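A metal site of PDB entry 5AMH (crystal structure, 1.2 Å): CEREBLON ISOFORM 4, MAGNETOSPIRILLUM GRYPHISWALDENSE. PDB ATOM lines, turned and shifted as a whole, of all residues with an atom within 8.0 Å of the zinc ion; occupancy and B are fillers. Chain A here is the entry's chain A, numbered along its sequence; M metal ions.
SG of Cys 28 is bound to the zinc ion, 2.3 Å away. The zinc ion is bound by SG of Cys 94. SG of Cys 25 binds the zinc ion. SG of Cys 91 binds the zinc ion (2.3 Å). The zinc ion has four donor atoms within binding distance.
The side-chain sulfur of Cys 28 lies close to the side-chain amide nitrogen of Gln 93, at 3.2 Å. The backbone NH (N) of Gln 30 sits close to the side-chain sulfur (SG) of Cys 28 (3.5 Å). N of Ser 96 sits close to SG of Cys 94 (3.4 Å). The backbone NH (N) of Gln 27 lies close to the side-chain sulfur (SG) of Cys 25, at 3.5 Å. The backbone NH of Cys 25 sits at hydrogen-bond distance from the backbone carbonyl oxygen of Gln 30. The backbone NH (N) of Cys 91 is in hydrogen-bond range of the backbone carbonyl oxygen (O) of Ser 96 (2.8 Å). The side-chain sulfur of Cys 91 lies close to the backbone NH of Gln 93, 3.5 Å away. The side-chain amide nitrogen (NE2) of Gln 30 lies close to the side-chain sulfur (SG) of Cys 91, 3.2 Å away.
Within 4 Å of the zinc ion: Cys 25, Cys 28, Cys 91 and Cys 94.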
ATOM      1  N   ARG A  24     -19.880 -13.132  25.046  1.00  0.00           N
ATOM      2  CA  ARG A  24     -18.607 -13.290  24.356  1.00  0.00           C
ATOM      3  C   ARG A  24     -17.620 -13.997  25.284  1.00  0.00           C
ATOM      4  O   ARG A  24     -17.721 -13.907  26.517  1.00  0.00           O
ATOM      5  CB  ARG A  24     -18.062 -11.932  23.953  1.00  0.00           C
ATOM      6  CG  ARG A  24     -18.919 -11.225  22.967  1.00  0.00           C
ATOM      7  CD  ARG A  24     -18.347  -9.891  22.535  1.00  0.00           C
ATOM      8  NE  ARG A  24     -19.195  -9.214  21.510  1.00  0.00           N
ATOM      9  CZ  ARG A  24     -20.263  -8.484  21.759  1.00  0.00           C
ATOM     10  NH1 ARG A  24     -20.611  -8.190  23.004  1.00  0.00           N
ATOM     11  NH2 ARG A  24     -20.954  -7.971  20.752  1.00  0.00           N
ATOM     12  N   CYS A  25     -16.635 -14.657  24.706  1.00  0.00           N
ATOM     13  CA  CYS A  25     -15.534 -15.220  25.455  1.00  0.00           C
ATOM     14  C   CYS A  25     -14.844 -14.076  26.198  1.00  0.00           C
ATOM     15  O   CYS A  25     -14.442 -13.081  25.583  1.00  0.00           O
ATOM     16  CB  CYS A  25     -14.541 -15.938  24.504  1.00  0.00           C
ATOM     17  SG  CYS A  25     -13.042 -16.487  25.324  1.00  0.00           S
ATOM     18  N   ARG A  26     -14.705 -14.192  27.528  1.00  0.00           N
ATOM     19  CA  ARG A  26     -14.084 -13.100  28.284  1.00  0.00           C
ATOM     20  C   ARG A  26     -12.611 -12.936  27.920  1.00  0.00           C
ATOM     21  O   ARG A  26     -12.077 -11.815  27.926  1.00  0.00           O
ATOM     22  CB  ARG A  26     -14.235 -13.325  29.785  1.00  0.00           C
ATOM     23  CG  ARG A  26     -13.693 -12.184  30.634  1.00  0.00           C
ATOM     24  CD  ARG A  26     -14.168 -12.330  32.089  1.00  0.00           C
ATOM     25  NE  ARG A  26     -15.578 -11.960  32.289  1.00  0.00           N
ATOM     26  CZ  ARG A  26     -16.041 -10.694  32.254  1.00  0.00           C
ATOM     27  NH1 ARG A  26     -15.199  -9.657  32.028  1.00  0.00           N
ATOM     28  NH2 ARG A  26     -17.321 -10.465  32.501  1.00  0.00           N
ATOM     29  N   GLN A  27     -11.942 -14.054  27.556  1.00  0.00           N
ATOM     30  CA  GLN A  27     -10.486 -14.019  27.204  1.00  0.00           C
ATOM     31  C   GLN A  27     -10.256 -13.318  25.876  1.00  0.00           C
ATOM     32  O   GLN A  27      -9.329 -12.514  25.798  1.00  0.00           O
ATOM     33  CB  GLN A  27      -9.929 -15.437  27.199  1.00  0.00           C
ATOM     34  CG  GLN A  27      -8.501 -15.590  26.914  1.00  0.00           C
ATOM     35  CD  GLN A  27      -7.661 -14.928  27.972  1.00  0.00           C
ATOM     36  OE1 GLN A  27      -7.641 -15.325  29.157  1.00  0.00           O
ATOM     37  NE2 GLN A  27      -7.074 -13.857  27.569  1.00  0.00           N
ATOM     38  N   CYS A  28     -11.016 -13.670  24.820  1.00  0.00           N
ATOM     39  CA  CYS A  28     -10.652 -13.197  23.483  1.00  0.00           C
ATOM     40  C   CYS A  28     -11.735 -12.362  22.765  1.00  0.00           C
ATOM     41  O   CYS A  28     -11.479 -11.830  21.692  1.00  0.00           O
ATOM     42  CB  CYS A  28     -10.203 -14.330  22.561  1.00  0.00           C
ATOM     43  SG  CYS A  28     -11.595 -15.339  21.943  1.00  0.00           S
ATOM     44  N   GLY A  29     -12.945 -12.345  23.328  1.00  0.00           N
ATOM     45  CA  GLY A  29     -14.026 -11.595  22.710  1.00  0.00           C
ATOM     46  C   GLY A  29     -14.842 -12.310  21.647  1.00  0.00           C
ATOM     47  O   GLY A  29     -15.796 -11.691  21.145  1.00  0.00           O
ATOM     48  N   GLN A  30     -14.544 -13.560  21.312  1.00  0.00           N
ATOM     49  CA  GLN A  30     -15.340 -14.231  20.338  1.00  0.00           C
ATOM     50  C   GLN A  30     -16.790 -14.340  20.784  1.00  0.00           C
ATOM     51  O   GLN A  30     -17.075 -14.633  21.939  1.00  0.00           O
ATOM     52  CB  GLN A  30     -14.808 -15.629  20.115  1.00  0.00           C
ATOM     53  CG  GLN A  30     -15.353 -16.134  18.835  1.00  0.00           C
ATOM     54  CD  GLN A  30     -15.268 -17.623  18.666  1.00  0.00           C
ATOM     55  OE1 GLN A  30     -15.477 -18.089  17.550  1.00  0.00           O
ATOM     56  NE2 GLN A  30     -15.008 -18.382  19.777  1.00  0.00           N
ATOM     57  N   THR A  31     -17.729 -14.184  19.825  1.00  0.00           N
ATOM     58  CA  THR A  31     -19.141 -14.420  20.104  1.00  0.00           C
ATOM     59  C   THR A  31     -19.433 -15.855  20.399  1.00  0.00           C
ATOM     60  O   THR A  31     -19.038 -16.758  19.624  1.00  0.00           O
ATOM     61  CB  THR A  31     -20.013 -13.907  18.941  1.00  0.00           C
ATOM     62  OG1 THR A  31     -19.826 -12.501  18.919  1.00  0.00           O
ATOM     63  CG2 THR A  31     -21.463 -14.308  19.120  1.00  0.00           C
ATOM     64  N   ILE A  32     -20.142 -16.108  21.521  1.00  0.00           N
ATOM     65  CA  ILE A  32     -20.446 -17.478  21.910  1.00  0.00           C
ATOM     66  C   ILE A  32     -21.961 -17.720  21.906  1.00  0.00           C
ATOM     67  O   ILE A  32     -22.445 -18.709  21.420  1.00  0.00           O
ATOM     68  CB  ILE A  32     -19.815 -17.823  23.256  1.00  0.00           C
ATOM     69  CG1 ILE A  32     -18.311 -17.608  23.247  1.00  0.00           C
ATOM     70  CG2 ILE A  32     -20.175 -19.244  23.684  1.00  0.00           C
ATOM     71  CD1 ILE A  32     -17.503 -18.475  22.341  1.00  0.00           C
ATOM     72  N   GLY A  67     -18.881 -20.985  18.235  1.00  0.00           N
ATOM     73  CA  GLY A  67     -17.520 -20.710  18.588  1.00  0.00           C
ATOM     74  C   GLY A  67     -16.841 -21.669  19.514  1.00  0.00           C
ATOM     75  O   GLY A  67     -15.845 -21.291  20.149  1.00  0.00           O
ATOM     76  N   LEU A  68     -17.344 -22.906  19.633  1.00  0.00           N
ATOM     77  CA  LEU A  68     -16.885 -23.845  20.640  1.00  0.00           C
ATOM     78  C   LEU A  68     -16.341 -25.102  20.015  1.00  0.00           C
ATOM     79  O   LEU A  68     -16.879 -25.673  19.066  1.00  0.00           O
ATOM     80  CB  LEU A  68     -18.032 -24.234  21.560  1.00  0.00           C
ATOM     81  CG  LEU A  68     -18.605 -23.109  22.371  1.00  0.00           C
ATOM     82  CD1 LEU A  68     -19.842 -23.598  23.132  1.00  0.00           C
ATOM     83  CD2 LEU A  68     -17.586 -22.544  23.363  1.00  0.00           C
ATOM     84  N   LEU A  90     -14.324 -25.709  24.818  1.00  0.00           N
ATOM     85  CA  LEU A  90     -13.315 -24.672  24.753  1.00  0.00           C
ATOM     86  C   LEU A  90     -13.709 -23.612  23.719  1.00  0.00           C
ATOM     87  O   LEU A  90     -14.293 -23.971  22.679  1.00  0.00           O
ATOM     88  CB  LEU A  90     -11.964 -25.243  24.345  1.00  0.00           C
ATOM     89  CG  LEU A  90     -11.381 -26.358  25.218  1.00  0.00           C
ATOM     90  CD1 LEU A  90     -10.002 -26.715  24.728  1.00  0.00           C
ATOM     91  CD2 LEU A  90     -11.341 -25.994  26.682  1.00  0.00           C
ATOM     92  N   CYS A  91     -13.335 -22.385  23.948  1.00  0.00           N
ATOM     93  CA  CYS A  91     -13.417 -21.363  22.899  1.00  0.00           C
ATOM     94  C   CYS A  91     -12.583 -21.817  21.722  1.00  0.00           C
ATOM     95  O   CYS A  91     -11.384 -22.133  21.888  1.00  0.00           O
ATOM     96  CB  CYS A  91     -12.859 -20.067  23.429  1.00  0.00           C
ATOM     97  SG  CYS A  91     -12.899 -18.752  22.181  1.00  0.00           S
ATOM     98  N   GLY A  92     -13.138 -21.865  20.527  1.00  0.00           N
ATOM     99  CA  GLY A  92     -12.370 -22.288  19.365  1.00  0.00           C
ATOM    100  C   GLY A  92     -11.248 -21.288  19.033  1.00  0.00           C
ATOM    101  O   GLY A  92     -10.196 -21.735  18.502  1.00  0.00           O
ATOM    102  N   GLN A  93     -11.413 -20.035  19.301  1.00  0.00           N
ATOM    103  CA  GLN A  93     -10.384 -19.098  18.955  1.00  0.00           C
ATOM    104  C   GLN A  93      -9.195 -19.116  19.892  1.00  0.00           C
ATOM    105  O   GLN A  93      -8.053 -19.102  19.411  1.00  0.00           O
ATOM    106  CB  GLN A  93     -10.951 -17.700  18.860  1.00  0.00           C
ATOM    107  CG  GLN A  93      -9.936 -16.660  18.427  1.00  0.00           C
ATOM    108  CD  GLN A  93     -10.583 -15.432  17.932  1.00  0.00           C
ATOM    109  OE1 GLN A  93     -10.594 -15.180  16.707  1.00  0.00           O
ATOM    110  NE2 GLN A  93     -11.196 -14.738  18.779  1.00  0.00           N
ATOM    111  N   CYS A  94      -9.458 -19.077  21.188  1.00  0.00           N
ATOM    112  CA  CYS A  94      -8.353 -18.936  22.170  1.00  0.00           C
ATOM    113  C   CYS A  94      -8.142 -20.085  23.067  1.00  0.00           C
ATOM    114  O   CYS A  94      -7.146 -20.104  23.820  1.00  0.00           O
ATOM    115  CB  CYS A  94      -8.550 -17.665  23.003  1.00  0.00           C
ATOM    116  SG  CYS A  94      -9.796 -17.844  24.303  1.00  0.00           S
ATOM    117  N   GLY A  95      -9.019 -21.094  23.050  1.00  0.00           N
ATOM    118  CA  GLY A  95      -8.871 -22.232  23.890  1.00  0.00           C
ATOM    119  C   GLY A  95      -9.282 -22.106  25.340  1.00  0.00           C
ATOM    120  O   GLY A  95      -9.112 -23.060  26.097  1.00  0.00           O
ATOM    121  N   SER A  96      -9.860 -20.962  25.704  1.00  0.00           N
ATOM    122  CA  SER A  96     -10.347 -20.834  27.067  1.00  0.00           C
ATOM    123  C   SER A  96     -11.406 -21.894  27.374  1.00  0.00           C
ATOM    124  O   SER A  96     -12.211 -22.230  26.506  1.00  0.00           O
ATOM    125  CB  SER A  96     -10.972 -19.455  27.267  1.00  0.00           C
ATOM    126  OG  SER A  96     -11.511 -19.245  28.519  1.00  0.00           O
ATOM    127  N   HIS A  97     -11.418 -22.421  28.608  1.00  0.00           N
ATOM    128  CA  HIS A  97     -12.419 -23.354  29.000  1.00  0.00           C
ATOM    129  C   HIS A  97     -13.683 -22.645  29.419  1.00  0.00           C
ATOM    130  O   HIS A  97     -13.790 -22.091  30.494  1.00  0.00           O
ATOM    131  CB  HIS A  97     -11.889 -24.263  30.126  1.00  0.00           C
ATOM    132  CG  HIS A  97     -12.862 -25.298  30.533  1.00  0.00           C
ATOM    133  ND1 HIS A  97     -12.751 -25.983  31.706  1.00  0.00           N
ATOM    134  CD2 HIS A  97     -14.018 -25.699  29.970  1.00  0.00           C
ATOM    135  CE1 HIS A  97     -13.800 -26.807  31.872  1.00  0.00           C
ATOM    136  NE2 HIS A  97     -14.580 -26.613  30.824  1.00  0.00           N
ATOM    137  N   LEU A  98     -14.666 -22.610  28.518  1.00  0.00           N
ATOM    138  CA  LEU A  98     -15.883 -21.845  28.691  1.00  0.00           C
ATOM    139  C   LEU A  98     -16.966 -22.618  29.388  1.00  0.00           C
ATOM    140  O   LEU A  98     -17.833 -22.007  30.058  1.00  0.00           O
ATOM    141  CB  LEU A  98     -16.396 -21.275  27.405  1.00  0.00           C
ATOM    142  CG  LEU A  98     -15.431 -20.334  26.674  1.00  0.00           C
ATOM    143  CD1 LEU A  98     -16.091 -19.732  25.481  1.00  0.00           C
ATOM    144  CD2 LEU A  98     -14.880 -19.266  27.549  1.00  0.00           C
ATOM    145  N   ARG A 118     -16.483 -16.849  32.832  1.00  0.00           N
ATOM    146  CA  ARG A 118     -15.649 -17.026  31.647  1.00  0.00           C
ATOM    147  C   ARG A 118     -16.231 -16.303  30.422  1.00  0.00           C
ATOM    148  O   ARG A 118     -15.614 -16.333  29.346  1.00  0.00           O
ATOM    149  CB  ARG A 118     -15.458 -18.508  31.368  1.00  0.00           C
ATOM    150  CG  ARG A 118     -14.815 -19.332  32.465  1.00  0.00           C
ATOM    151  CD  ARG A 118     -13.347 -19.386  32.417  1.00  0.00           C
ATOM    152  NE  ARG A 118     -12.867 -19.882  33.711  1.00  0.00           N
ATOM    153  CZ  ARG A 118     -12.708 -21.157  34.098  1.00  0.00           C
ATOM    154  NH1 ARG A 118     -12.846 -22.221  33.219  1.00  0.00           N
ATOM    155  NH2 ARG A 118     -12.436 -21.335  35.298  1.00  0.00           N
HETATM  156 ZN    ZN M   1     -11.810 -17.093  23.426  1.00  0.00          ZN
